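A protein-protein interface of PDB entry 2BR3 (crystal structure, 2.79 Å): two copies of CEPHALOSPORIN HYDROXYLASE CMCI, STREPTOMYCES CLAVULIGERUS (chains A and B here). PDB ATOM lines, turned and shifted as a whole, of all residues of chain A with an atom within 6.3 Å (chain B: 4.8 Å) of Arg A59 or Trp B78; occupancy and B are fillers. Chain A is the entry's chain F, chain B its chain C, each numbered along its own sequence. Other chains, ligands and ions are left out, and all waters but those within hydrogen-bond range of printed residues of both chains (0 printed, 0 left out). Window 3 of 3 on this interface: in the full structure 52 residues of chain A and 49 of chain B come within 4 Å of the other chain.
NH1 of Arg A59 sits at hydrogen-bond distance from O of Ile B105 (2.8 Å). The side-chain amide nitrogen (NE2) of Gln A57 is in hydrogen-bond range of the side-chain carboxylate (OD1) of Asp B75. The side-chain amide oxygen (OE1) of Gln A57 lies within hydrogen-bond range of a ring nitrogen (NE2) of His B74, 2.9 Å away. A ring nitrogen (NE2) of His B74 lies within hydrogen-bond range of the backbone NH (N) of Arg A59 (3.3 Å).
Printed residues of chain B within 4 Å of Gln A57: His B74 (2.9 Å), Asp B75 (3.1 Å) and Trp B78 (3.7 Å). Of chain B, only His B74, Trp B78 and Ile B105 come within 4 Å of Arg A59. Of the printed residues of chain A, His B74 touches Gln A57 (2.9 Å), Trp A58 (3.5 Å) and Arg A59 (3.3 Å). Of chain A, only Gln A57 (3.7 Å), Arg A59 (3.1 Å) and Gly A60 (3.6 Å) come within 4 Å of Trp B78. Of the printed residues of chain A, Ile B105 touches Trp A58 (3.3 Å), Arg A59 (2.8 Å) and Asp A101 (3.9 Å). The nearest residue of chain B that does not touch Arg A59 is Met B106 (4.4 Å). The nearest printed residue of chain B that does not touch Asp A101 is Met B106 (6.9 Å).
Among the printed residues, pairs that only touch across the chains: Gln A57 with Trp B78 (3.7 Å), Trp A58 with His B74 (3.5 Å), Trp A58 with Ile B105 (3.3 Å), Arg A59 with Trp B78 (3.1 Å), Gly A60 with Trp B78 (3.6 Å) and Asp A101 with Ile B105 (3.9 Å).
No position is printed for both chains.
Of the 10 printed residues of chain B, 4 touch a printed residue of chain A. Printed residues of chain B that touch a printed residue of chain A: His B74, Asp B75, Trp B78 and Ile B105. Hydrophobic or aromatic side chains of chain B that line the printed part of chain A: His B74, Trp B78 and Ile B105. Of the 10 printed residues of chain A, 5 touch a printed residue of chain B. Among the printed residues, 10 pairs touch across the chains.
The side-chain amide oxygen of Gln A57 is in hydrogen-bond range of the backbone NH of Gly A60, at 3.1 Å. The backbone NH (N) of Arg A59 sits at hydrogen-bond distance from the side-chain amide oxygen (OE1) of Gln A57, 3.1 Å away. OD2 of Asp A101 sits at hydrogen-bond distance from NE1 of Trp A58 (2.9 Å). The guanidinium group (NH2) of Arg A59 lies within salt-bridge range of the side-chain carboxylate (OD1) of Asp A128 (3.1 Å). The guanidinium group of Arg A100 is in salt-bridge range of the side-chain carboxylate of Asp A101, 3.1 Å away. The guanidinium group (NE) of Arg A59 is in salt-bridge range of the side-chain carboxylate (OD2) of Asp A101 (2.9 Å).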
ATOM      1  N   TYR A  24      -3.928 -23.831  12.425  1.00  0.00           N
ATOM      2  CA  TYR A  24      -4.846 -23.948  11.295  1.00  0.00           C
ATOM      3  C   TYR A  24      -5.478 -25.326  11.213  1.00  0.00           C
ATOM      4  O   TYR A  24      -4.811 -26.318  11.439  1.00  0.00           O
ATOM      5  CB  TYR A  24      -4.083 -23.693   9.988  1.00  0.00           C
ATOM      6  CG  TYR A  24      -4.944 -23.831   8.752  1.00  0.00           C
ATOM      7  CD1 TYR A  24      -6.012 -22.959   8.530  1.00  0.00           C
ATOM      8  CD2 TYR A  24      -4.708 -24.837   7.816  1.00  0.00           C
ATOM      9  CE1 TYR A  24      -6.816 -23.076   7.416  1.00  0.00           C
ATOM     10  CE2 TYR A  24      -5.510 -24.961   6.687  1.00  0.00           C
ATOM     11  CZ  TYR A  24      -6.564 -24.076   6.501  1.00  0.00           C
ATOM     12  OH  TYR A  24      -7.372 -24.172   5.396  1.00  0.00           O
ATOM     13  N   GLN A  57      -5.287 -19.005   5.342  1.00  0.00           N
ATOM     14  CA  GLN A  57      -4.012 -19.583   5.774  1.00  0.00           C
ATOM     15  C   GLN A  57      -2.864 -19.311   4.820  1.00  0.00           C
ATOM     16  O   GLN A  57      -3.069 -18.929   3.674  1.00  0.00           O
ATOM     17  CB  GLN A  57      -4.139 -21.094   5.935  1.00  0.00           C
ATOM     18  CG  GLN A  57      -4.539 -21.806   4.660  1.00  0.00           C
ATOM     19  CD  GLN A  57      -3.574 -22.895   4.248  1.00  0.00           C
ATOM     20  OE1 GLN A  57      -2.363 -22.698   4.277  1.00  0.00           O
ATOM     21  NE2 GLN A  57      -4.113 -24.047   3.848  1.00  0.00           N
ATOM     22  N   TRP A  58      -1.649 -19.514   5.323  1.00  0.00           N
ATOM     23  CA  TRP A  58      -0.437 -19.458   4.522  1.00  0.00           C
ATOM     24  C   TRP A  58       0.493 -20.566   4.994  1.00  0.00           C
ATOM     25  O   TRP A  58       1.089 -20.457   6.065  1.00  0.00           O
ATOM     26  CB  TRP A  58       0.246 -18.101   4.650  1.00  0.00           C
ATOM     27  CG  TRP A  58       1.475 -18.002   3.817  1.00  0.00           C
ATOM     28  CD1 TRP A  58       2.772 -18.142   4.239  1.00  0.00           C
ATOM     29  CD2 TRP A  58       1.542 -17.758   2.408  1.00  0.00           C
ATOM     30  NE1 TRP A  58       3.636 -17.995   3.179  1.00  0.00           N
ATOM     31  CE2 TRP A  58       2.909 -17.760   2.041  1.00  0.00           C
ATOM     32  CE3 TRP A  58       0.583 -17.525   1.411  1.00  0.00           C
ATOM     33  CZ2 TRP A  58       3.337 -17.539   0.733  1.00  0.00           C
ATOM     34  CZ3 TRP A  58       1.011 -17.310   0.105  1.00  0.00           C
ATOM     35  CH2 TRP A  58       2.378 -17.320  -0.220  1.00  0.00           C
ATOM     36  N   ARG A  59       0.565 -21.642   4.202  1.00  0.00           N
ATOM     37  CA  ARG A  59       1.486 -22.760   4.414  1.00  0.00           C
ATOM     38  C   ARG A  59       1.218 -23.551   5.693  1.00  0.00           C
ATOM     39  O   ARG A  59       2.148 -23.986   6.355  1.00  0.00           O
ATOM     40  CB  ARG A  59       2.934 -22.263   4.399  1.00  0.00           C
ATOM     41  CG  ARG A  59       3.245 -21.357   3.235  1.00  0.00           C
ATOM     42  CD  ARG A  59       4.697 -21.376   2.796  1.00  0.00           C
ATOM     43  NE  ARG A  59       5.597 -20.898   3.847  1.00  0.00           N
ATOM     44  CZ  ARG A  59       6.712 -21.517   4.243  1.00  0.00           C
ATOM     45  NH1 ARG A  59       7.090 -22.672   3.696  1.00  0.00           N
ATOM     46  NH2 ARG A  59       7.454 -20.983   5.209  1.00  0.00           N
ATOM     47  N   GLY A  60      -0.049 -23.757   6.030  1.00  0.00           N
ATOM     48  CA  GLY A  60      -0.406 -24.440   7.261  1.00  0.00           C
ATOM     49  C   GLY A  60      -0.410 -23.535   8.481  1.00  0.00           C
ATOM     50  O   GLY A  60      -0.533 -24.021   9.606  1.00  0.00           O
ATOM     51  N   LEU A  61      -0.270 -22.227   8.263  1.00  0.00           N
ATOM     52  CA  LEU A  61      -0.438 -21.222   9.321  1.00  0.00           C
ATOM     53  C   LEU A  61      -1.691 -20.389   9.053  1.00  0.00           C
ATOM     54  O   LEU A  61      -2.005 -20.082   7.913  1.00  0.00           O
ATOM     55  CB  LEU A  61       0.777 -20.282   9.403  1.00  0.00           C
ATOM     56  CG  LEU A  61       2.163 -20.905   9.613  1.00  0.00           C
ATOM     57  CD1 LEU A  61       3.232 -19.815   9.702  1.00  0.00           C
ATOM     58  CD2 LEU A  61       2.189 -21.790  10.859  1.00  0.00           C
ATOM     59  N   ALA A  97       5.345 -14.618   8.891  1.00  0.00           N
ATOM     60  CA  ALA A  97       5.903 -15.558   7.935  1.00  0.00           C
ATOM     61  C   ALA A  97       5.569 -15.120   6.521  1.00  0.00           C
ATOM     62  O   ALA A  97       6.425 -15.170   5.645  1.00  0.00           O
ATOM     63  CB  ALA A  97       5.376 -16.969   8.200  1.00  0.00           C
ATOM     64  N   ARG A 100       7.622 -12.252   5.272  1.00  0.00           N
ATOM     65  CA  ARG A 100       8.966 -12.761   5.005  1.00  0.00           C
ATOM     66  C   ARG A 100       9.028 -13.518   3.678  1.00  0.00           C
ATOM     67  O   ARG A 100       9.918 -13.263   2.866  1.00  0.00           O
ATOM     68  CB  ARG A 100       9.456 -13.675   6.139  1.00  0.00           C
ATOM     69  CG  ARG A 100      10.949 -14.070   6.042  1.00  0.00           C
ATOM     70  CD  ARG A 100      11.260 -15.347   5.247  1.00  0.00           C
ATOM     71  NE  ARG A 100      10.309 -16.433   5.503  1.00  0.00           N
ATOM     72  CZ  ARG A 100      10.349 -17.263   6.548  1.00  0.00           C
ATOM     73  NH1 ARG A 100      11.295 -17.156   7.479  1.00  0.00           N
ATOM     74  NH2 ARG A 100       9.424 -18.212   6.663  1.00  0.00           N
ATOM     75  N   ASP A 101       8.097 -14.445   3.457  1.00  0.00           N
ATOM     76  CA  ASP A 101       8.131 -15.255   2.246  1.00  0.00           C
ATOM     77  C   ASP A 101       8.024 -14.345   1.032  1.00  0.00           C
ATOM     78  O   ASP A 101       8.889 -14.356   0.177  1.00  0.00           O
ATOM     79  CB  ASP A 101       7.031 -16.319   2.249  1.00  0.00           C
ATOM     80  CG  ASP A 101       7.358 -17.492   3.156  1.00  0.00           C
ATOM     81  OD1 ASP A 101       8.543 -17.811   3.345  1.00  0.00           O
ATOM     82  OD2 ASP A 101       6.493 -18.174   3.727  1.00  0.00           O
ATOM     83  N   ASP A 128      12.244 -22.385  10.752  1.00  0.00           N
ATOM     84  CA  ASP A 128      11.598 -21.642   9.673  1.00  0.00           C
ATOM     85  C   ASP A 128      11.506 -20.154  10.053  1.00  0.00           C
ATOM     86  O   ASP A 128      10.531 -19.476   9.736  1.00  0.00           O
ATOM     87  CB  ASP A 128      10.210 -22.246   9.408  1.00  0.00           C
ATOM     88  CG  ASP A 128       9.559 -21.709   8.143  1.00  0.00           C
ATOM     89  OD1 ASP A 128       8.322 -21.864   8.021  1.00  0.00           O
ATOM     90  OD2 ASP A 128      10.194 -21.120   7.233  1.00  0.00           O
ATOM     91  N   HIS B  74      -4.248 -21.414  -3.410  1.00  0.00           N
ATOM     92  CA  HIS B  74      -3.273 -21.590  -2.349  1.00  0.00           C
ATOM     93  C   HIS B  74      -3.637 -22.838  -1.551  1.00  0.00           C
ATOM     94  O   HIS B  74      -2.828 -23.737  -1.403  1.00  0.00           O
ATOM     95  CB  HIS B  74      -3.222 -20.397  -1.396  1.00  0.00           C
ATOM     96  CG  HIS B  74      -2.455 -20.701  -0.155  1.00  0.00           C
ATOM     97  ND1 HIS B  74      -1.079 -20.632  -0.102  1.00  0.00           N
ATOM     98  CD2 HIS B  74      -2.857 -21.171   1.048  1.00  0.00           C
ATOM     99  CE1 HIS B  74      -0.667 -21.006   1.094  1.00  0.00           C
ATOM    100  NE2 HIS B  74      -1.726 -21.337   1.813  1.00  0.00           N
ATOM    101  N   ASP B  75      -4.861 -22.875  -1.040  1.00  0.00           N
ATOM    102  CA  ASP B  75      -5.344 -24.006  -0.259  1.00  0.00           C
ATOM    103  C   ASP B  75      -5.223 -25.311  -1.013  1.00  0.00           C
ATOM    104  O   ASP B  75      -4.800 -26.307  -0.437  1.00  0.00           O
ATOM    105  CB  ASP B  75      -6.809 -23.802   0.123  1.00  0.00           C
ATOM    106  CG  ASP B  75      -6.981 -22.846   1.283  1.00  0.00           C
ATOM    107  OD1 ASP B  75      -5.963 -22.451   1.880  1.00  0.00           O
ATOM    108  OD2 ASP B  75      -8.095 -22.447   1.677  1.00  0.00           O
ATOM    109  N   MET B  76      -5.579 -25.297  -2.297  1.00  0.00           N
ATOM    110  CA  MET B  76      -5.618 -26.511  -3.120  1.00  0.00           C
ATOM    111  C   MET B  76      -4.211 -27.078  -3.253  1.00  0.00           C
ATOM    112  O   MET B  76      -3.977 -28.252  -2.960  1.00  0.00           O
ATOM    113  CB  MET B  76      -6.200 -26.198  -4.505  1.00  0.00           C
ATOM    114  CG  MET B  76      -6.589 -27.419  -5.364  1.00  0.00           C
ATOM    115  SD  MET B  76      -7.228 -26.957  -7.028  1.00  0.00           S
ATOM    116  CE  MET B  76      -8.770 -26.182  -6.595  1.00  0.00           C
ATOM    117  N   LEU B  77      -3.280 -26.220  -3.670  1.00  0.00           N
ATOM    118  CA  LEU B  77      -1.862 -26.570  -3.789  1.00  0.00           C
ATOM    119  C   LEU B  77      -1.305 -27.205  -2.526  1.00  0.00           C
ATOM    120  O   LEU B  77      -0.582 -28.193  -2.602  1.00  0.00           O
ATOM    121  CB  LEU B  77      -1.030 -25.326  -4.120  1.00  0.00           C
ATOM    122  CG  LEU B  77      -0.815 -24.990  -5.600  1.00  0.00           C
ATOM    123  CD1 LEU B  77      -2.050 -25.218  -6.456  1.00  0.00           C
ATOM    124  CD2 LEU B  77      -0.371 -23.555  -5.705  1.00  0.00           C
ATOM    125  N   TRP B  78      -1.645 -26.630  -1.374  1.00  0.00           N
ATOM    126  CA  TRP B  78      -1.135 -27.083  -0.078  1.00  0.00           C
ATOM    127  C   TRP B  78      -1.684 -28.450   0.322  1.00  0.00           C
ATOM    128  O   TRP B  78      -0.983 -29.249   0.943  1.00  0.00           O
ATOM    129  CB  TRP B  78      -1.483 -26.064   1.001  1.00  0.00           C
ATOM    130  CG  TRP B  78      -1.022 -26.441   2.366  1.00  0.00           C
ATOM    131  CD1 TRP B  78      -1.786 -26.930   3.390  1.00  0.00           C
ATOM    132  CD2 TRP B  78       0.311 -26.354   2.866  1.00  0.00           C
ATOM    133  NE1 TRP B  78      -1.005 -27.150   4.501  1.00  0.00           N
ATOM    134  CE2 TRP B  78       0.289 -26.804   4.207  1.00  0.00           C
ATOM    135  CE3 TRP B  78       1.535 -25.937   2.319  1.00  0.00           C
ATOM    136  CZ2 TRP B  78       1.438 -26.855   5.004  1.00  0.00           C
ATOM    137  CZ3 TRP B  78       2.683 -25.989   3.117  1.00  0.00           C
ATOM    138  CH2 TRP B  78       2.621 -26.443   4.443  1.00  0.00           C
ATOM    139  N   GLU B  79      -2.934 -28.714  -0.039  1.00  0.00           N
ATOM    140  CA  GLU B  79      -3.545 -30.014   0.195  1.00  0.00           C
ATOM    141  C   GLU B  79      -3.033 -31.060  -0.806  1.00  0.00           C
ATOM    142  O   GLU B  79      -2.680 -32.183  -0.439  1.00  0.00           O
ATOM    143  CB  GLU B  79      -5.071 -29.905   0.092  1.00  0.00           C
ATOM    144  CG  GLU B  79      -5.805 -30.903   0.974  1.00  0.00           C
ATOM    145  CD  GLU B  79      -7.226 -31.182   0.526  1.00  0.00           C
ATOM    146  OE1 GLU B  79      -7.739 -30.473  -0.367  1.00  0.00           O
ATOM    147  OE2 GLU B  79      -7.832 -32.123   1.078  1.00  0.00           O
ATOM    148  N   LEU B  80      -2.969 -30.675  -2.071  1.00  0.00           N
ATOM    149  CA  LEU B  80      -2.796 -31.630  -3.153  1.00  0.00           C
ATOM    150  C   LEU B  80      -1.316 -31.917  -3.444  1.00  0.00           C
ATOM    151  O   LEU B  80      -0.962 -33.012  -3.892  1.00  0.00           O
ATOM    152  CB  LEU B  80      -3.502 -31.087  -4.401  1.00  0.00           C
ATOM    153  CG  LEU B  80      -3.981 -32.016  -5.527  1.00  0.00           C
ATOM    154  CD1 LEU B  80      -2.987 -31.978  -6.666  1.00  0.00           C
ATOM    155  CD2 LEU B  80      -4.254 -33.455  -5.073  1.00  0.00           C
ATOM    156  N   ARG B  81      -0.462 -30.936  -3.172  1.00  0.00           N
ATOM    157  CA  ARG B  81       0.966 -31.010  -3.495  1.00  0.00           C
ATOM    158  C   ARG B  81       1.213 -31.517  -4.939  1.00  0.00           C
ATOM    159  O   ARG B  81       1.844 -32.554  -5.159  1.00  0.00           O
ATOM    160  CB  ARG B  81       1.706 -31.854  -2.452  1.00  0.00           C
ATOM    161  CG  ARG B  81       1.695 -31.239  -1.060  1.00  0.00           C
ATOM    162  CD  ARG B  81       2.622 -31.916  -0.074  1.00  0.00           C
ATOM    163  NE  ARG B  81       4.018 -31.606  -0.368  1.00  0.00           N
ATOM    164  CZ  ARG B  81       4.718 -30.591   0.145  1.00  0.00           C
ATOM    165  NH1 ARG B  81       4.170 -29.748   1.014  1.00  0.00           N
ATOM    166  NH2 ARG B  81       5.990 -30.422  -0.220  1.00  0.00           N
ATOM    167  N   ILE B 105       7.811 -21.793  -2.597  1.00  0.00           N
ATOM    168  CA  ILE B 105       7.854 -21.439  -1.167  1.00  0.00           C
ATOM    169  C   ILE B 105       7.196 -22.507  -0.292  1.00  0.00           C
ATOM    170  O   ILE B 105       7.524 -22.627   0.886  1.00  0.00           O
ATOM    171  CB  ILE B 105       7.257 -20.022  -0.830  1.00  0.00           C
ATOM    172  CG1 ILE B 105       6.501 -19.407  -2.006  1.00  0.00           C
ATOM    173  CG2 ILE B 105       8.380 -19.076  -0.360  1.00  0.00           C
ATOM    174  CD1 ILE B 105       5.584 -18.295  -1.618  1.00  0.00           C
ATOM    175  N   MET B 106       6.281 -23.278  -0.865  1.00  0.00           N
ATOM    176  CA  MET B 106       5.737 -24.444  -0.182  1.00  0.00           C
ATOM    177  C   MET B 106       6.688 -25.622  -0.265  1.00  0.00           C
ATOM    178  O   MET B 106       6.475 -26.625   0.406  1.00  0.00           O
ATOM    179  CB  MET B 106       4.406 -24.850  -0.794  1.00  0.00           C
ATOM    180  CG  MET B 106       3.309 -23.834  -0.593  1.00  0.00           C
ATOM    181  SD  MET B 106       1.960 -24.161  -1.713  1.00  0.00           S
ATOM    182  CE  MET B 106       0.669 -23.079  -1.005  1.00  0.00           C
